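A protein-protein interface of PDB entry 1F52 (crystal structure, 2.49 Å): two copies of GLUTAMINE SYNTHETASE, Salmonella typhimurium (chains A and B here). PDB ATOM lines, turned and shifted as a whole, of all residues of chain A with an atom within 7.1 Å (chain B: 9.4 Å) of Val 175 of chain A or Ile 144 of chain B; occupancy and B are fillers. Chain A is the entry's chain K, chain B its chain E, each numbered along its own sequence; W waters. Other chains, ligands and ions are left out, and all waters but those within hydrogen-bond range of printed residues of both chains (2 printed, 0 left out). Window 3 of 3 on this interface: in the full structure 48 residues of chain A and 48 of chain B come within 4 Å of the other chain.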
ATOM      1  N   ILE A 151      10.385  26.850  -2.452  1.00  0.00           N
ATOM      2  CA  ILE A 151      11.214  27.318  -1.348  1.00  0.00           C
ATOM      3  C   ILE A 151      11.826  26.151  -0.633  1.00  0.00           C
ATOM      4  O   ILE A 151      11.190  25.097  -0.509  1.00  0.00           O
ATOM      5  CB  ILE A 151      10.366  28.072  -0.336  1.00  0.00           C
ATOM      6  CG1 ILE A 151       9.900  29.403  -0.935  1.00  0.00           C
ATOM      7  CG2 ILE A 151      11.146  28.306   0.956  1.00  0.00           C
ATOM      8  CD1 ILE A 151       8.595  29.915  -0.365  1.00  0.00           C
ATOM      9  N   ALA A 157       9.558  22.482   7.874  1.00  0.00           N
ATOM     10  CA  ALA A 157       8.917  21.311   8.441  1.00  0.00           C
ATOM     11  C   ALA A 157       8.740  20.191   7.426  1.00  0.00           C
ATOM     12  O   ALA A 157       8.816  19.006   7.779  1.00  0.00           O
ATOM     13  CB  ALA A 157       7.598  21.687   9.030  1.00  0.00           C
ATOM     14  N   TRP A 158       8.555  20.566   6.163  1.00  0.00           N
ATOM     15  CA  TRP A 158       8.351  19.588   5.102  1.00  0.00           C
ATOM     16  C   TRP A 158       9.529  18.655   4.910  1.00  0.00           C
ATOM     17  O   TRP A 158       9.379  17.579   4.345  1.00  0.00           O
ATOM     18  CB  TRP A 158       8.018  20.280   3.777  1.00  0.00           C
ATOM     19  CG  TRP A 158       9.027  21.292   3.339  1.00  0.00           C
ATOM     20  CD1 TRP A 158      10.159  21.062   2.608  1.00  0.00           C
ATOM     21  CD2 TRP A 158       8.990  22.702   3.586  1.00  0.00           C
ATOM     22  NE1 TRP A 158      10.831  22.245   2.384  1.00  0.00           N
ATOM     23  CE2 TRP A 158      10.127  23.269   2.973  1.00  0.00           C
ATOM     24  CE3 TRP A 158       8.096  23.544   4.268  1.00  0.00           C
ATOM     25  CZ2 TRP A 158      10.402  24.643   3.012  1.00  0.00           C
ATOM     26  CZ3 TRP A 158       8.370  24.918   4.309  1.00  0.00           C
ATOM     27  CH2 TRP A 158       9.512  25.450   3.683  1.00  0.00           C
ATOM     28  N   ARG A 172      13.460  20.112  13.698  1.00  0.00           N
ATOM     29  CA  ARG A 172      12.985  21.265  12.970  1.00  0.00           C
ATOM     30  C   ARG A 172      11.789  21.923  13.601  1.00  0.00           C
ATOM     31  O   ARG A 172      10.946  21.273  14.215  1.00  0.00           O
ATOM     32  CB  ARG A 172      12.563  20.846  11.566  1.00  0.00           C
ATOM     33  CG  ARG A 172      13.647  20.197  10.777  1.00  0.00           C
ATOM     34  CD  ARG A 172      13.178  19.792   9.410  1.00  0.00           C
ATOM     35  NE  ARG A 172      14.351  19.476   8.598  1.00  0.00           N
ATOM     36  CZ  ARG A 172      15.018  18.330   8.706  1.00  0.00           C
ATOM     37  NH1 ARG A 172      16.094  18.102   7.956  1.00  0.00           N
ATOM     38  NH2 ARG A 172      14.582  17.389   9.541  1.00  0.00           N
ATOM     39  N   PRO A 173      11.668  23.231  13.395  1.00  0.00           N
ATOM     40  CA  PRO A 173      10.562  24.009  13.923  1.00  0.00           C
ATOM     41  C   PRO A 173       9.357  23.638  13.081  1.00  0.00           C
ATOM     42  O   PRO A 173       9.441  23.619  11.854  1.00  0.00           O
ATOM     43  CB  PRO A 173      11.008  25.447  13.651  1.00  0.00           C
ATOM     44  CG  PRO A 173      11.854  25.327  12.446  1.00  0.00           C
ATOM     45  CD  PRO A 173      12.663  24.104  12.750  1.00  0.00           C
ATOM     46  N   GLY A 174       8.267  23.244  13.728  1.00  0.00           N
ATOM     47  CA  GLY A 174       7.069  22.899  12.982  1.00  0.00           C
ATOM     48  C   GLY A 174       6.409  24.161  12.454  1.00  0.00           C
ATOM     49  O   GLY A 174       6.904  25.263  12.690  1.00  0.00           O
ATOM     50  N   VAL A 175       5.297  24.019  11.742  1.00  0.00           N
ATOM     51  CA  VAL A 175       4.599  25.182  11.201  1.00  0.00           C
ATOM     52  C   VAL A 175       4.141  26.060  12.368  1.00  0.00           C
ATOM     53  O   VAL A 175       3.570  25.551  13.336  1.00  0.00           O
ATOM     54  CB  VAL A 175       3.408  24.732  10.318  1.00  0.00           C
ATOM     55  CG1 VAL A 175       2.611  25.926   9.836  1.00  0.00           C
ATOM     56  CG2 VAL A 175       3.929  23.942   9.119  1.00  0.00           C
ATOM     57  N   LYS A 176       4.440  27.361  12.289  1.00  0.00           N
ATOM     58  CA  LYS A 176       4.110  28.334  13.344  1.00  0.00           C
ATOM     59  C   LYS A 176       4.779  27.943  14.672  1.00  0.00           C
ATOM     60  O   LYS A 176       4.385  28.423  15.737  1.00  0.00           O
ATOM     61  CB  LYS A 176       2.584  28.465  13.559  1.00  0.00           C
ATOM     62  CG  LYS A 176       1.791  29.166  12.441  1.00  0.00           C
ATOM     63  CD  LYS A 176       0.278  29.137  12.723  1.00  0.00           C
ATOM     64  CE  LYS A 176      -0.571  29.078  11.440  1.00  0.00           C
ATOM     65  NZ  LYS A 176      -0.511  30.315  10.601  1.00  0.00           N
ATOM     66  N   GLY A 177       5.800  27.093  14.625  1.00  0.00           N
ATOM     67  CA  GLY A 177       6.432  26.643  15.864  1.00  0.00           C
ATOM     68  C   GLY A 177       7.892  27.127  16.046  1.00  0.00           C
ATOM     69  O   GLY A 177       8.681  26.478  16.732  1.00  0.00           O
ATOM     70  N   GLY A 178       8.224  28.262  15.453  1.00  0.00           N
ATOM     71  CA  GLY A 178       9.573  28.775  15.543  1.00  0.00           C
ATOM     72  C   GLY A 178       9.828  29.652  16.749  1.00  0.00           C
ATOM     73  O   GLY A 178      10.978  29.969  17.031  1.00  0.00           O
ATOM     74  N   VAL A 213       8.327  33.241  14.343  1.00  0.00           N
ATOM     75  CA  VAL A 213       7.328  32.189  14.388  1.00  0.00           C
ATOM     76  C   VAL A 213       7.363  31.121  13.300  1.00  0.00           C
ATOM     77  O   VAL A 213       7.244  29.931  13.617  1.00  0.00           O
ATOM     78  CB  VAL A 213       5.934  32.819  14.355  1.00  0.00           C
ATOM     79  CG1 VAL A 213       4.857  31.744  14.302  1.00  0.00           C
ATOM     80  CG2 VAL A 213       5.716  33.726  15.550  1.00  0.00           C
ATOM     81  N   ALA A 214       7.526  31.514  12.067  1.00  0.00           N
ATOM     82  CA  ALA A 214       7.435  30.564  10.965  1.00  0.00           C
ATOM     83  C   ALA A 214       8.530  29.511  10.907  1.00  0.00           C
ATOM     84  O   ALA A 214       9.657  29.729  11.352  1.00  0.00           O
ATOM     85  CB  ALA A 214       7.388  31.326   9.657  1.00  0.00           C
ATOM     86  N   THR A 215       8.173  28.352  10.362  1.00  0.00           N
ATOM     87  CA  THR A 215       9.129  27.278  10.152  1.00  0.00           C
ATOM     88  C   THR A 215      10.012  27.784   9.005  1.00  0.00           C
ATOM     89  O   THR A 215       9.775  28.848   8.439  1.00  0.00           O
ATOM     90  CB  THR A 215       8.430  25.999   9.722  1.00  0.00           C
ATOM     91  OG1 THR A 215       9.398  24.977   9.481  1.00  0.00           O
ATOM     92  CG2 THR A 215       7.636  26.253   8.455  1.00  0.00           C
ATOM     93  N   ALA A 216      11.036  27.035   8.658  1.00  0.00           N
ATOM     94  CA  ALA A 216      11.836  27.408   7.516  1.00  0.00           C
ATOM     95  C   ALA A 216      12.614  28.727   7.626  1.00  0.00           C
ATOM     96  O   ALA A 216      12.741  29.442   6.622  1.00  0.00           O
ATOM     97  CB  ALA A 216      10.936  27.463   6.295  1.00  0.00           C
ATOM     98  N   PRO A 259       6.161  34.928   2.016  1.00  0.00           N
ATOM     99  CA  PRO A 259       6.663  33.954   1.045  1.00  0.00           C
ATOM    100  C   PRO A 259       5.905  32.638   1.089  1.00  0.00           C
ATOM    101  O   PRO A 259       5.857  31.904   0.094  1.00  0.00           O
ATOM    102  CB  PRO A 259       8.126  33.785   1.449  1.00  0.00           C
ATOM    103  CG  PRO A 259       8.097  34.007   2.935  1.00  0.00           C
ATOM    104  CD  PRO A 259       7.144  35.173   3.095  1.00  0.00           C
ATOM    105  N   MET A 260       5.256  32.354   2.212  1.00  0.00           N
ATOM    106  CA  MET A 260       4.521  31.103   2.334  1.00  0.00           C
ATOM    107  C   MET A 260       3.097  31.215   2.822  1.00  0.00           C
ATOM    108  O   MET A 260       2.812  31.904   3.798  1.00  0.00           O
ATOM    109  CB  MET A 260       5.252  30.151   3.281  1.00  0.00           C
ATOM    110  CG  MET A 260       6.652  29.783   2.854  1.00  0.00           C
ATOM    111  SD  MET A 260       7.429  28.765   4.099  1.00  0.00           S
ATOM    112  CE  MET A 260       7.935  30.016   5.264  1.00  0.00           C
ATOM    113  N   PHE A 261       2.233  30.496   2.134  1.00  0.00           N
ATOM    114  CA  PHE A 261       0.853  30.466   2.561  1.00  0.00           C
ATOM    115  C   PHE A 261       0.784  29.460   3.718  1.00  0.00           C
ATOM    116  O   PHE A 261       1.296  28.360   3.573  1.00  0.00           O
ATOM    117  CB  PHE A 261      -0.113  30.057   1.451  1.00  0.00           C
ATOM    118  CG  PHE A 261      -1.484  29.795   2.016  1.00  0.00           C
ATOM    119  CD1 PHE A 261      -2.310  30.873   2.287  1.00  0.00           C
ATOM    120  CD2 PHE A 261      -1.928  28.520   2.326  1.00  0.00           C
ATOM    121  CE1 PHE A 261      -3.567  30.689   2.873  1.00  0.00           C
ATOM    122  CE2 PHE A 261      -3.185  28.321   2.910  1.00  0.00           C
ATOM    123  CZ  PHE A 261      -4.003  29.417   3.186  1.00  0.00           C
ATOM    124  N   GLY A 262       0.155  29.798   4.835  1.00  0.00           N
ATOM    125  CA  GLY A 262       0.058  28.809   5.893  1.00  0.00           C
ATOM    126  C   GLY A 262       0.943  29.030   7.092  1.00  0.00           C
ATOM    127  O   GLY A 262       0.884  28.268   8.058  1.00  0.00           O
ATOM    128  N   ASP A 263       1.841  29.997   6.993  1.00  0.00           N
ATOM    129  CA  ASP A 263       2.687  30.311   8.119  1.00  0.00           C
ATOM    130  C   ASP A 263       2.888  31.807   8.092  1.00  0.00           C
ATOM    131  O   ASP A 263       2.517  32.487   7.130  1.00  0.00           O
ATOM    132  CB  ASP A 263       4.025  29.560   8.079  1.00  0.00           C
ATOM    133  CG  ASP A 263       4.586  29.289   9.483  1.00  0.00           C
ATOM    134  OD1 ASP A 263       5.339  28.308   9.670  1.00  0.00           O
ATOM    135  OD2 ASP A 263       4.267  30.047  10.416  1.00  0.00           O
ATOM    136  N   ASN A 264       3.438  32.309   9.186  1.00  0.00           N
ATOM    137  CA  ASN A 264       3.699  33.719   9.385  1.00  0.00           C
ATOM    138  C   ASN A 264       4.300  34.464   8.225  1.00  0.00           C
ATOM    139  O   ASN A 264       5.100  33.921   7.470  1.00  0.00           O
ATOM    140  CB  ASN A 264       4.670  33.864  10.538  1.00  0.00           C
ATOM    141  CG  ASN A 264       4.132  34.705  11.636  1.00  0.00           C
ATOM    142  OD1 ASN A 264       4.787  35.652  12.089  1.00  0.00           O
ATOM    143  ND2 ASN A 264       2.941  34.352  12.110  1.00  0.00           N
ATOM    144  N   GLY B 141       0.119  22.359  -8.519  1.00  0.00           N
ATOM    145  CA  GLY B 141       0.052  22.067  -7.108  1.00  0.00           C
ATOM    146  C   GLY B 141       0.357  23.311  -6.303  1.00  0.00           C
ATOM    147  O   GLY B 141       0.790  24.330  -6.846  1.00  0.00           O
ATOM    148  N   ALA B 142       0.105  23.232  -5.004  1.00  0.00           N
ATOM    149  CA  ALA B 142       0.364  24.336  -4.104  1.00  0.00           C
ATOM    150  C   ALA B 142       0.385  23.775  -2.710  1.00  0.00           C
ATOM    151  O   ALA B 142      -0.490  23.005  -2.328  1.00  0.00           O
ATOM    152  CB  ALA B 142      -0.701  25.374  -4.223  1.00  0.00           C
ATOM    153  N   SER B 143       1.456  24.084  -2.000  1.00  0.00           N
ATOM    154  CA  SER B 143       1.621  23.631  -0.637  1.00  0.00           C
ATOM    155  C   SER B 143       2.342  24.754   0.073  1.00  0.00           C
ATOM    156  O   SER B 143       2.608  25.805  -0.513  1.00  0.00           O
ATOM    157  CB  SER B 143       2.437  22.345  -0.574  1.00  0.00           C
ATOM    158  OG  SER B 143       3.778  22.558  -0.958  1.00  0.00           O
ATOM    159  N   ILE B 144       2.683  24.532   1.329  1.00  0.00           N
ATOM    160  CA  ILE B 144       3.328  25.580   2.081  1.00  0.00           C
ATOM    161  C   ILE B 144       4.634  26.064   1.464  1.00  0.00           C
ATOM    162  O   ILE B 144       4.907  27.259   1.454  1.00  0.00           O
ATOM    163  CB  ILE B 144       3.562  25.126   3.524  1.00  0.00           C
ATOM    164  CG1 ILE B 144       4.119  26.269   4.350  1.00  0.00           C
ATOM    165  CG2 ILE B 144       4.519  23.953   3.565  1.00  0.00           C
ATOM    166  CD1 ILE B 144       4.146  25.975   5.810  1.00  0.00           C
ATOM    167  N   SER B 145       5.402  25.153   0.882  1.00  0.00           N
ATOM    168  CA  SER B 145       6.692  25.530   0.335  1.00  0.00           C
ATOM    169  C   SER B 145       6.704  26.030  -1.088  1.00  0.00           C
ATOM    170  O   SER B 145       7.775  26.217  -1.658  1.00  0.00           O
ATOM    171  CB  SER B 145       7.682  24.390   0.480  1.00  0.00           C
ATOM    172  OG  SER B 145       7.280  23.309  -0.326  1.00  0.00           O
ATOM    173  N   GLY B 146       5.534  26.212  -1.686  1.00  0.00           N
ATOM    174  CA  GLY B 146       5.513  26.747  -3.036  1.00  0.00           C
ATOM    175  C   GLY B 146       4.275  26.382  -3.811  1.00  0.00           C
ATOM    176  O   GLY B 146       3.281  25.919  -3.243  1.00  0.00           O
ATOM    177  N   SER B 147       4.339  26.553  -5.102  1.00  0.00           N
ATOM    178  CA  SER B 147       3.217  26.238  -5.984  1.00  0.00           C
ATOM    179  C   SER B 147       3.692  26.303  -7.417  1.00  0.00           C
ATOM    180  O   SER B 147       4.738  26.894  -7.713  1.00  0.00           O
ATOM    181  CB  SER B 147       2.058  27.202  -5.793  1.00  0.00           C
ATOM    182  OG  SER B 147       2.448  28.538  -6.065  1.00  0.00           O
ATOM    183  N   ARG B 452      -8.634  31.790  -1.952  1.00  0.00           N
ATOM    184  CA  ARG B 452      -7.496  30.921  -2.183  1.00  0.00           C
ATOM    185  C   ARG B 452      -6.485  31.666  -3.028  1.00  0.00           C
ATOM    186  O   ARG B 452      -5.299  31.707  -2.725  1.00  0.00           O
ATOM    187  CB  ARG B 452      -7.930  29.685  -2.949  1.00  0.00           C
ATOM    188  CG  ARG B 452      -8.868  28.755  -2.221  1.00  0.00           C
ATOM    189  CD  ARG B 452      -8.141  27.935  -1.190  1.00  0.00           C
ATOM    190  NE  ARG B 452      -6.863  27.426  -1.676  1.00  0.00           N
ATOM    191  CZ  ARG B 452      -6.719  26.334  -2.420  1.00  0.00           C
ATOM    192  NH1 ARG B 452      -5.494  25.965  -2.797  1.00  0.00           N
ATOM    193  NH2 ARG B 452      -7.785  25.617  -2.777  1.00  0.00           N
ATOM    194  N   THR B 456      -2.813  33.006  -1.457  1.00  0.00           N
ATOM    195  CA  THR B 456      -1.648  32.191  -1.791  1.00  0.00           C
ATOM    196  C   THR B 456      -0.597  32.953  -2.572  1.00  0.00           C
ATOM    197  O   THR B 456      -0.891  33.517  -3.619  1.00  0.00           O
ATOM    198  CB  THR B 456      -2.054  30.982  -2.609  1.00  0.00           C
ATOM    199  OG1 THR B 456      -3.120  30.281  -1.945  1.00  0.00           O
ATOM    200  CG2 THR B 456      -0.873  30.068  -2.776  1.00  0.00           C
ATOM    201  N   PRO B 457       0.650  32.985  -2.072  1.00  0.00           N
ATOM    202  CA  PRO B 457       1.704  33.707  -2.788  1.00  0.00           C
ATOM    203  C   PRO B 457       1.767  33.276  -4.233  1.00  0.00           C
ATOM    204  O   PRO B 457       1.594  32.104  -4.542  1.00  0.00           O
ATOM    205  CB  PRO B 457       2.958  33.295  -2.043  1.00  0.00           C
ATOM    206  CG  PRO B 457       2.465  33.205  -0.620  1.00  0.00           C
ATOM    207  CD  PRO B 457       1.138  32.474  -0.779  1.00  0.00           C
ATOM    208  N   PHE B 462       7.575  36.475  -6.364  1.00  0.00           N
ATOM    209  CA  PHE B 462       8.982  36.188  -6.015  1.00  0.00           C
ATOM    210  C   PHE B 462       9.914  36.900  -6.983  1.00  0.00           C
ATOM    211  O   PHE B 462      10.922  37.477  -6.587  1.00  0.00           O
ATOM    212  CB  PHE B 462       9.226  34.671  -6.018  1.00  0.00           C
ATOM    213  CG  PHE B 462       8.486  34.074  -4.860  1.00  0.00           C
ATOM    214  CD1 PHE B 462       9.112  33.853  -3.654  1.00  0.00           C
ATOM    215  CD2 PHE B 462       7.135  33.796  -4.964  1.00  0.00           C
ATOM    216  CE1 PHE B 462       8.404  33.373  -2.558  1.00  0.00           C
ATOM    217  CE2 PHE B 462       6.423  33.317  -3.872  1.00  0.00           C
ATOM    218  CZ  PHE B 462       7.062  33.110  -2.670  1.00  0.00           C
HETATM  219  O   HOH W   1      -0.075  25.489   2.894  1.00  0.00           O
HETATM  220  O   HOH W   2       3.136  28.777   0.146  1.00  0.00           O
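Among the printed residues, pairs that only touch across the chains: Pro 259 of chain A with Phe 462 of chain B, Met 260 of chain A with Ile 144 of chain B, Phe 261 of chain A with Pro 457 of chain B, Phe 261 of chain A with Ile 144 of chain B, Trp 158 of chain A with Ser 145 of chain B, Trp 158 of chain A with Ile 144 of chain B, Pro 259 of chain A with Pro 457 of chain B and Val 175 of chain A with Ile 144 of chain B.
O of Ser 145 of chain B is in hydrogen-bond range of N of Ile 151 of chain A (2.8 Å).
Of the 11 printed residues of chain B, 4 touch a printed residue of chain A.
Printed residues of chain B that touch a printed residue of chain A: Ile 144, Ser 145, Pro 457 and Phe 462.
Among the printed residues, 9 pairs touch across the chains.
Among the printed residues, no Asp or Glu carboxylate lies within 4 Å of a Lys or Arg side-chain nitrogen of the other chain.
No position is printed for both chains.
Of the 9 pairs that touch across the chains among the printed residues, none has its exchanged pair printed and touching as well.
Val 175 of chain A touches just one residue of chain B: Ile 144.
Of the printed residues of chain A, Ile 144 of chain B touches Trp 158, Val 175, Met 260 and Phe 261.
Gly 174 of chain A touches none of the printed residues of chain B.
No residue of chain B comes within 4 Å of Gly 262 of chain A.
Of the printed residues of chain B, Trp 158 of chain A touches Ile 144 and Ser 145.
Printed residues of chain A within 4 Å of Pro 457 of chain B: Pro 259 (3.7 Å) and Phe 261 (3.5 Å).
Printed residues of chain B within 4 Å of Met 260 of chain A: Ile 144 (3.4 Å).
Ala 142 of chain B touches none of the printed residues of chain A.
The nearest residue of chain B that does not touch Val 175 of chain A is Ser 145 of chain B (8.5 Å).
Water W2 lies within hydrogen-bond range of O of Ile 144 of chain B (2.7 Å), N of Phe 261 of chain A (2.8 Å) and O of Ser 143 of chain B (3.1 Å).
Water W1 lies within hydrogen-bond range of the backbone carbonyl oxygen (O) of Phe 261 of chain A (3.3 Å) and the backbone NH (N) of Ile 144 of chain B (3.3 Å).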
